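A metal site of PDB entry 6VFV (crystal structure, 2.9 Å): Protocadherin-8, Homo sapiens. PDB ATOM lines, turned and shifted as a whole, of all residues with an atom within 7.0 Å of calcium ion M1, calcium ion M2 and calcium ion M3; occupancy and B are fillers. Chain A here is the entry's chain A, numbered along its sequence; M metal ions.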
ATOM      1  N   GLU A  19      24.026   4.176  16.402  1.00  0.00           N
ATOM      2  CA  GLU A  19      24.279   3.363  15.219  1.00  0.00           C
ATOM      3  C   GLU A  19      25.445   2.407  15.441  1.00  0.00           C
ATOM      4  O   GLU A  19      26.333   2.641  16.271  1.00  0.00           O
ATOM      5  CB  GLU A  19      24.558   4.298  14.035  1.00  0.00           C
ATOM      6  CG  GLU A  19      24.783   3.636  12.703  1.00  0.00           C
ATOM      7  CD  GLU A  19      25.223   4.640  11.651  1.00  0.00           C
ATOM      8  OE1 GLU A  19      25.416   5.824  12.005  1.00  0.00           O
ATOM      9  OE2 GLU A  19      25.370   4.241  10.477  1.00  0.00           O
ATOM     10  N   ASN A  20      25.443   1.311  14.684  1.00  0.00           N
ATOM     11  CA  ASN A  20      26.526   0.323  14.692  1.00  0.00           C
ATOM     12  C   ASN A  20      26.690  -0.310  16.077  1.00  0.00           C
ATOM     13  O   ASN A  20      27.806  -0.460  16.593  1.00  0.00           O
ATOM     14  CB  ASN A  20      27.840   0.947  14.217  1.00  0.00           C
ATOM     15  CG  ASN A  20      27.700   1.653  12.871  1.00  0.00           C
ATOM     16  OD1 ASN A  20      27.114   1.114  11.926  1.00  0.00           O
ATOM     17  ND2 ASN A  20      28.222   2.864  12.786  1.00  0.00           N
ATOM     18  N   PHE A  78      22.459  -1.535  14.077  1.00  0.00           N
ATOM     19  CA  PHE A  78      21.579  -0.598  13.392  1.00  0.00           C
ATOM     20  C   PHE A  78      22.402   0.419  12.603  1.00  0.00           C
ATOM     21  O   PHE A  78      23.426   0.906  13.080  1.00  0.00           O
ATOM     22  CB  PHE A  78      20.674   0.124  14.393  1.00  0.00           C
ATOM     23  CG  PHE A  78      19.795  -0.801  15.191  1.00  0.00           C
ATOM     24  CD1 PHE A  78      19.611  -0.613  16.547  1.00  0.00           C
ATOM     25  CD2 PHE A  78      19.132  -1.859  14.570  1.00  0.00           C
ATOM     26  CE1 PHE A  78      18.795  -1.465  17.275  1.00  0.00           C
ATOM     27  CE2 PHE A  78      18.320  -2.703  15.294  1.00  0.00           C
ATOM     28  CZ  PHE A  78      18.149  -2.510  16.649  1.00  0.00           C
ATOM     29  N   ASP A  79      21.929   0.723  11.401  1.00  0.00           N
ATOM     30  CA  ASP A  79      22.558   1.697  10.507  1.00  0.00           C
ATOM     31  C   ASP A  79      21.640   2.912  10.382  1.00  0.00           C
ATOM     32  O   ASP A  79      20.526   2.800   9.862  1.00  0.00           O
ATOM     33  CB  ASP A  79      22.830   1.079   9.136  1.00  0.00           C
ATOM     34  CG  ASP A  79      23.370   2.089   8.146  1.00  0.00           C
ATOM     35  OD1 ASP A  79      23.900   3.128   8.586  1.00  0.00           O
ATOM     36  OD2 ASP A  79      23.282   1.819   6.924  1.00  0.00           O
ATOM     37  N   TYR A  80      22.109   4.059  10.868  1.00  0.00           N
ATOM     38  CA  TYR A  80      21.262   5.253  10.889  1.00  0.00           C
ATOM     39  C   TYR A  80      20.916   5.699   9.474  1.00  0.00           C
ATOM     40  O   TYR A  80      19.789   6.147   9.215  1.00  0.00           O
ATOM     41  CB  TYR A  80      21.962   6.378  11.654  1.00  0.00           C
ATOM     42  CG  TYR A  80      21.195   7.685  11.644  1.00  0.00           C
ATOM     43  CD1 TYR A  80      20.202   7.933  12.577  1.00  0.00           C
ATOM     44  CD2 TYR A  80      21.461   8.666  10.699  1.00  0.00           C
ATOM     45  CE1 TYR A  80      19.497   9.117  12.578  1.00  0.00           C
ATOM     46  CE2 TYR A  80      20.758   9.852  10.677  1.00  0.00           C
ATOM     47  CZ  TYR A  80      19.773  10.074  11.618  1.00  0.00           C
ATOM     48  OH  TYR A  80      19.084  11.265  11.594  1.00  0.00           O
ATOM     49  N   GLU A  81      21.859   5.597   8.543  1.00  0.00           N
ATOM     50  CA  GLU A  81      21.578   5.974   7.163  1.00  0.00           C
ATOM     51  C   GLU A  81      20.522   5.071   6.533  1.00  0.00           C
ATOM     52  O   GLU A  81      19.932   5.433   5.523  1.00  0.00           O
ATOM     53  CB  GLU A  81      22.864   5.943   6.335  1.00  0.00           C
ATOM     54  CG  GLU A  81      23.822   7.103   6.612  1.00  0.00           C
ATOM     55  CD  GLU A  81      24.511   7.000   7.964  1.00  0.00           C
ATOM     56  OE1 GLU A  81      25.167   5.970   8.225  1.00  0.00           O
ATOM     57  OE2 GLU A  81      24.379   7.946   8.769  1.00  0.00           O
ATOM     58  N   THR A  82      20.270   3.899   7.125  1.00  0.00           N
ATOM     59  CA  THR A  82      19.292   2.941   6.620  1.00  0.00           C
ATOM     60  C   THR A  82      17.997   2.928   7.410  1.00  0.00           C
ATOM     61  O   THR A  82      16.964   2.524   6.856  1.00  0.00           O
ATOM     62  CB  THR A  82      19.917   1.531   6.633  1.00  0.00           C
ATOM     63  OG1 THR A  82      20.924   1.437   5.619  1.00  0.00           O
ATOM     64  CG2 THR A  82      18.866   0.438   6.407  1.00  0.00           C
ATOM     65  N   LEU A 111      20.451   6.804  16.951  1.00  0.00           N
ATOM     66  CA  LEU A 111      21.268   8.002  16.895  1.00  0.00           C
ATOM     67  C   LEU A 111      22.415   7.810  15.909  1.00  0.00           C
ATOM     68  O   LEU A 111      22.851   6.684  15.644  1.00  0.00           O
ATOM     69  CB  LEU A 111      21.834   8.349  18.268  1.00  0.00           C
ATOM     70  CG  LEU A 111      20.848   8.412  19.425  1.00  0.00           C
ATOM     71  CD1 LEU A 111      21.579   8.186  20.726  1.00  0.00           C
ATOM     72  CD2 LEU A 111      20.124   9.739  19.436  1.00  0.00           C
ATOM     73  N   ASP A 112      22.901   8.920  15.387  1.00  0.00           N
ATOM     74  CA  ASP A 112      23.941   8.891  14.371  1.00  0.00           C
ATOM     75  C   ASP A 112      25.315   8.733  15.011  1.00  0.00           C
ATOM     76  O   ASP A 112      25.578   9.183  16.130  1.00  0.00           O
ATOM     77  CB  ASP A 112      23.898  10.161  13.525  1.00  0.00           C
ATOM     78  CG  ASP A 112      24.921  10.154  12.410  1.00  0.00           C
ATOM     79  OD1 ASP A 112      25.251   9.057  11.905  1.00  0.00           O
ATOM     80  OD2 ASP A 112      25.401  11.246  12.030  1.00  0.00           O
ATOM     81  N   GLN A 113      26.196   8.061  14.281  1.00  0.00           N
ATOM     82  CA  GLN A 113      27.605   7.894  14.616  1.00  0.00           C
ATOM     83  C   GLN A 113      28.414   8.412  13.435  1.00  0.00           C
ATOM     84  O   GLN A 113      28.003   8.288  12.284  1.00  0.00           O
ATOM     85  CB  GLN A 113      27.912   6.416  14.902  1.00  0.00           C
ATOM     86  CG  GLN A 113      29.303   6.078  15.428  1.00  0.00           C
ATOM     87  CD  GLN A 113      29.477   4.576  15.681  1.00  0.00           C
ATOM     88  OE1 GLN A 113      28.520   3.819  15.574  1.00  0.00           O
ATOM     89  NE2 GLN A 113      30.687   4.169  16.014  1.00  0.00           N
ATOM     90  N   ASN A 114      29.562   9.035  13.712  1.00  0.00           N
ATOM     91  CA  ASN A 114      30.410   9.531  12.628  1.00  0.00           C
ATOM     92  C   ASN A 114      31.177   8.337  12.058  1.00  0.00           C
ATOM     93  O   ASN A 114      32.328   8.059  12.399  1.00  0.00           O
ATOM     94  CB  ASN A 114      31.348  10.628  13.095  1.00  0.00           C
ATOM     95  CG  ASN A 114      31.945  11.417  11.935  1.00  0.00           C
ATOM     96  OD1 ASN A 114      31.473  11.309  10.806  1.00  0.00           O
ATOM     97  ND2 ASN A 114      32.974  12.206  12.204  1.00  0.00           N
ATOM     98  N   ASP A 115      30.496   7.615  11.157  1.00  0.00           N
ATOM     99  CA  ASP A 115      31.038   6.414  10.538  1.00  0.00           C
ATOM    100  C   ASP A 115      31.213   6.615   9.031  1.00  0.00           C
ATOM    101  O   ASP A 115      31.135   5.656   8.250  1.00  0.00           O
ATOM    102  CB  ASP A 115      30.156   5.202  10.825  1.00  0.00           C
ATOM    103  CG  ASP A 115      28.743   5.391  10.347  1.00  0.00           C
ATOM    104  OD1 ASP A 115      28.291   6.556  10.265  1.00  0.00           O
ATOM    105  OD2 ASP A 115      28.074   4.380  10.048  1.00  0.00           O
ATOM    106  N   HIS A 116      31.431   7.850   8.601  1.00  0.00           N
ATOM    107  CA  HIS A 116      31.713   8.165   7.208  1.00  0.00           C
ATOM    108  C   HIS A 116      32.775   9.247   7.153  1.00  0.00           C
ATOM    109  O   HIS A 116      32.588  10.343   7.697  1.00  0.00           O
ATOM    110  CB  HIS A 116      30.456   8.609   6.447  1.00  0.00           C
ATOM    111  CG  HIS A 116      29.564   7.478   6.049  1.00  0.00           C
ATOM    112  ND1 HIS A 116      28.330   7.269   6.610  1.00  0.00           N
ATOM    113  CD2 HIS A 116      29.733   6.504   5.123  1.00  0.00           C
ATOM    114  CE1 HIS A 116      27.762   6.209   6.054  1.00  0.00           C
ATOM    115  NE2 HIS A 116      28.595   5.733   5.143  1.00  0.00           N
ATOM    116  N   ALA A 117      33.853   8.959   6.528  1.00  0.00           N
ATOM    117  CA  ALA A 117      34.802  10.013   6.229  1.00  0.00           C
ATOM    118  C   ALA A 117      34.413  10.698   4.924  1.00  0.00           C
ATOM    119  O   ALA A 117      33.813  10.073   4.049  1.00  0.00           O
ATOM    120  CB  ALA A 117      36.211   9.437   6.112  1.00  0.00           C
ATOM    121  N   PRO A 118      34.720  11.983   4.764  1.00  0.00           N
ATOM    122  CA  PRO A 118      34.397  12.648   3.500  1.00  0.00           C
ATOM    123  C   PRO A 118      35.039  11.919   2.327  1.00  0.00           C
ATOM    124  O   PRO A 118      36.141  11.402   2.421  1.00  0.00           O
ATOM    125  CB  PRO A 118      34.961  14.060   3.676  1.00  0.00           C
ATOM    126  CG  PRO A 118      35.903  13.971   4.841  1.00  0.00           C
ATOM    127  CD  PRO A 118      35.378  12.889   5.715  1.00  0.00           C
ATOM    128  N   ASP A 151      29.629  13.686   2.351  1.00  0.00           N
ATOM    129  CA  ASP A 151      29.669  12.996   3.629  1.00  0.00           C
ATOM    130  C   ASP A 151      28.245  12.634   4.013  1.00  0.00           C
ATOM    131  O   ASP A 151      27.369  13.504   4.042  1.00  0.00           O
ATOM    132  CB  ASP A 151      30.315  13.871   4.706  1.00  0.00           C
ATOM    133  CG  ASP A 151      30.642  13.104   5.990  1.00  0.00           C
ATOM    134  OD1 ASP A 151      29.812  12.257   6.413  1.00  0.00           O
ATOM    135  OD2 ASP A 151      31.714  13.343   6.570  1.00  0.00           O
ATOM    136  N   ALA A 152      28.017  11.364   4.297  1.00  0.00           N
ATOM    137  CA  ALA A 152      26.663  10.853   4.500  1.00  0.00           C
ATOM    138  C   ALA A 152      26.115  11.124   5.887  1.00  0.00           C
ATOM    139  O   ALA A 152      24.899  10.977   6.081  1.00  0.00           O
ATOM    140  CB  ALA A 152      26.642   9.351   4.236  1.00  0.00           C
ATOM    141  N   ASP A 153      26.950  11.514   6.843  1.00  0.00           N
ATOM    142  CA  ASP A 153      26.524  11.603   8.232  1.00  0.00           C
ATOM    143  C   ASP A 153      25.641  12.837   8.444  1.00  0.00           C
ATOM    144  O   ASP A 153      25.296  13.561   7.511  1.00  0.00           O
ATOM    145  CB  ASP A 153      27.751  11.606   9.142  1.00  0.00           C
ATOM    146  CG  ASP A 153      28.558  10.323   9.047  1.00  0.00           C
ATOM    147  OD1 ASP A 153      27.944   9.225   8.980  1.00  0.00           O
ATOM    148  OD2 ASP A 153      29.808  10.402   9.039  1.00  0.00           O
ATOM    149  N   GLU A 154      25.270  13.065   9.702  1.00  0.00           N
ATOM    150  CA  GLU A 154      24.307  14.092  10.079  1.00  0.00           C
ATOM    151  C   GLU A 154      25.006  15.251  10.771  1.00  0.00           C
ATOM    152  O   GLU A 154      26.114  15.129  11.290  1.00  0.00           O
ATOM    153  CB  GLU A 154      23.235  13.488  10.997  1.00  0.00           C
ATOM    154  CG  GLU A 154      22.280  14.492  11.623  1.00  0.00           C
ATOM    155  CD  GLU A 154      21.133  13.830  12.366  1.00  0.00           C
ATOM    156  OE1 GLU A 154      21.191  12.605  12.567  1.00  0.00           O
ATOM    157  OE2 GLU A 154      20.183  14.549  12.763  1.00  0.00           O
ATOM    158  N   ALA A 156      27.044  18.260  12.112  1.00  0.00           N
ATOM    159  CA  ALA A 156      28.445  18.592  11.876  1.00  0.00           C
ATOM    160  C   ALA A 156      29.216  17.409  11.312  1.00  0.00           C
ATOM    161  O   ALA A 156      30.217  17.604  10.600  1.00  0.00           O
ATOM    162  CB  ALA A 156      29.106  19.076  13.176  1.00  0.00           C
ATOM    163  N   ASN A 157      28.783  16.175  11.595  1.00  0.00           N
ATOM    164  CA  ASN A 157      29.441  15.010  11.016  1.00  0.00           C
ATOM    165  C   ASN A 157      29.381  14.986   9.496  1.00  0.00           C
ATOM    166  O   ASN A 157      30.076  14.179   8.877  1.00  0.00           O
ATOM    167  CB  ASN A 157      28.828  13.716  11.565  1.00  0.00           C
ATOM    168  CG  ASN A 157      29.122  13.508  13.039  1.00  0.00           C
ATOM    169  OD1 ASN A 157      30.206  13.848  13.523  1.00  0.00           O
ATOM    170  ND2 ASN A 157      28.167  12.937  13.757  1.00  0.00           N
ATOM    171  N   GLY A 158      28.564  15.834   8.885  1.00  0.00           N
ATOM    172  CA  GLY A 158      28.536  15.972   7.438  1.00  0.00           C
ATOM    173  C   GLY A 158      28.946  17.363   6.995  1.00  0.00           C
ATOM    174  O   GLY A 158      28.944  17.671   5.798  1.00  0.00           O
ATOM    175  N   GLU A 159      29.307  18.215   7.960  1.00  0.00           N
ATOM    176  CA  GLU A 159      29.729  19.583   7.669  1.00  0.00           C
ATOM    177  C   GLU A 159      31.202  19.571   7.268  1.00  0.00           C
ATOM    178  O   GLU A 159      32.080  19.339   8.105  1.00  0.00           O
ATOM    179  CB  GLU A 159      29.490  20.473   8.890  1.00  0.00           C
ATOM    180  CG  GLU A 159      29.663  21.951   8.643  1.00  0.00           C
ATOM    181  CD  GLU A 159      29.246  22.796   9.842  1.00  0.00           C
ATOM    182  OE1 GLU A 159      29.021  22.225  10.931  1.00  0.00           O
ATOM    183  OE2 GLU A 159      29.147  24.033   9.684  1.00  0.00           O
ATOM    184  N   LEU A 160      31.480  19.822   5.989  1.00  0.00           N
ATOM    185  CA  LEU A 160      32.814  19.673   5.433  1.00  0.00           C
ATOM    186  C   LEU A 160      33.579  20.995   5.418  1.00  0.00           C
ATOM    187  O   LEU A 160      33.005  22.082   5.403  1.00  0.00           O
ATOM    188  CB  LEU A 160      32.747  19.110   4.016  1.00  0.00           C
ATOM    189  CG  LEU A 160      32.212  17.671   3.877  1.00  0.00           C
ATOM    190  CD1 LEU A 160      32.645  17.086   2.533  1.00  0.00           C
ATOM    191  CD2 LEU A 160      32.673  16.777   5.030  1.00  0.00           C
ATOM    192  N   ASP A 205      35.610  16.831   8.227  1.00  0.00           N
ATOM    193  CA  ASP A 205      34.224  16.976   8.663  1.00  0.00           C
ATOM    194  C   ASP A 205      34.206  17.483  10.095  1.00  0.00           C
ATOM    195  O   ASP A 205      35.246  17.620  10.741  1.00  0.00           O
ATOM    196  CB  ASP A 205      33.458  15.654   8.510  1.00  0.00           C
ATOM    197  CG  ASP A 205      33.805  14.637   9.586  1.00  0.00           C
ATOM    198  OD1 ASP A 205      34.768  14.856  10.350  1.00  0.00           O
ATOM    199  OD2 ASP A 205      33.113  13.600   9.644  1.00  0.00           O
ATOM    200  N   GLY A 206      33.005  17.779  10.593  1.00  0.00           N
ATOM    201  CA  GLY A 206      32.891  18.457  11.867  1.00  0.00           C
ATOM    202  C   GLY A 206      32.730  17.533  13.057  1.00  0.00           C
ATOM    203  O   GLY A 206      32.081  17.891  14.040  1.00  0.00           O
ATOM    204  N   GLY A 207      33.312  16.338  12.978  1.00  0.00           N
ATOM    205  CA  GLY A 207      33.236  15.398  14.081  1.00  0.00           C
ATOM    206  C   GLY A 207      34.194  15.737  15.208  1.00  0.00           C
ATOM    207  O   GLY A 207      35.062  16.609  15.110  1.00  0.00           O
ATOM    208  N   LEU A 211      36.882  13.231  11.042  1.00  0.00           N
ATOM    209  CA  LEU A 211      37.387  12.295  10.051  1.00  0.00           C
ATOM    210  C   LEU A 211      37.903  13.076   8.848  1.00  0.00           C
ATOM    211  O   LEU A 211      37.191  13.917   8.303  1.00  0.00           O
ATOM    212  CB  LEU A 211      36.316  11.296   9.629  1.00  0.00           C
ATOM    213  CG  LEU A 211      35.873  10.287  10.695  1.00  0.00           C
ATOM    214  CD1 LEU A 211      35.112   9.144  10.057  1.00  0.00           C
ATOM    215  CD2 LEU A 211      37.050   9.733  11.496  1.00  0.00           C
HETATM  216 CA    CA M   1      26.445   7.828  10.401  1.00  0.00          CA
HETATM  217 CA    CA M   2      26.104   3.546   8.571  1.00  0.00          CA
HETATM  218 CA    CA M   3      31.490  12.240   8.661  1.00  0.00          CA
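Calcium ion M3 is bound by the side-chain carboxylate (OD2) of Asp 205.
OD1 of Asn 114 binds calcium ion M3 (2.3 Å).
Calcium ion M3 is bound by OD2 of Asp 151 (2.4 Å).
O of His 116 is bound to calcium ion M3 (2.4 Å).
O of Asn 157 binds calcium ion M3 (2.4 Å).
The side-chain carboxylate (OD2) of Asp 153 is bound to calcium ion M3, at 2.5 Å.
OD1 of Asp 151 binds calcium ion M3, 2.8 Å away.
Calcium ion M2 is bound by the side-chain carboxylate of Glu 19 (2.2 Å), the side-chain carboxylate of Asp 79 (2.2 Å), the side-chain carboxylate of Asp 115 (2.6 Å) and the side-chain carboxylate of Glu 81 (2.6 Å).
Calcium ion M2 has four donor atoms within binding distance.
Of the 28 residues printed, 6 come within 4 Å of calcium ion M1.
The side-chain carboxylate (OE2) of Glu 19 sits close to the backbone NH (N) of Tyr 80, at 3.3 Å.
The side-chain carboxylate (OD2) of Asp 79 sits at hydrogen-bond distance from the side-chain hydroxyl (OG1) of Thr 82, at 2.7 Å.
The backbone NH (N) of Glu 154 lies within hydrogen-bond range of the side-chain carboxylate (OD2) of Asp 112.
The backbone NH of Glu 19 sits at hydrogen-bond distance from the backbone carbonyl oxygen of Leu 111 (2.9 Å).
The side-chain carboxylate (OD2) of Asp 115 lies close to the side-chain amide nitrogen (ND2) of Asn 20 (3.1 Å).
The side-chain carboxylate (OD1) of Asp 205 sits close to the backbone NH (N) of Gly 207 (3.4 Å).
The backbone NH of Leu 211 lies within hydrogen-bond range of the side-chain carboxylate of Asp 205 (2.8 Å).
The side-chain amide oxygen (OE1) of Gln 113 is in hydrogen-bond range of the side-chain amide nitrogen (ND2) of Asn 20, 3.0 Å away.
Calcium ion M1 is bound by the side-chain carboxylate of Asp 115 (2.2 Å), the side-chain carboxylate of Asp 112 (2.3 Å), the backbone carbonyl oxygen of Gln 113 (2.5 Å), the side-chain carboxylate of Asp 153 (2.5 Å), the side-chain carboxylate of Glu 81 (2.6 Å) and the side-chain carboxylate of Glu 19 (2.8 Å).
Calcium ion M1 has six donor atoms within binding distance.
Slightly farther from calcium ion M1 lies OE1 of Glu 81 (3.1 Å).
Of the 28 residues printed, 4 come within 4 Å of calcium ion M2.
Of the 28 residues printed, 6 come within 4 Å of calcium ion M3.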
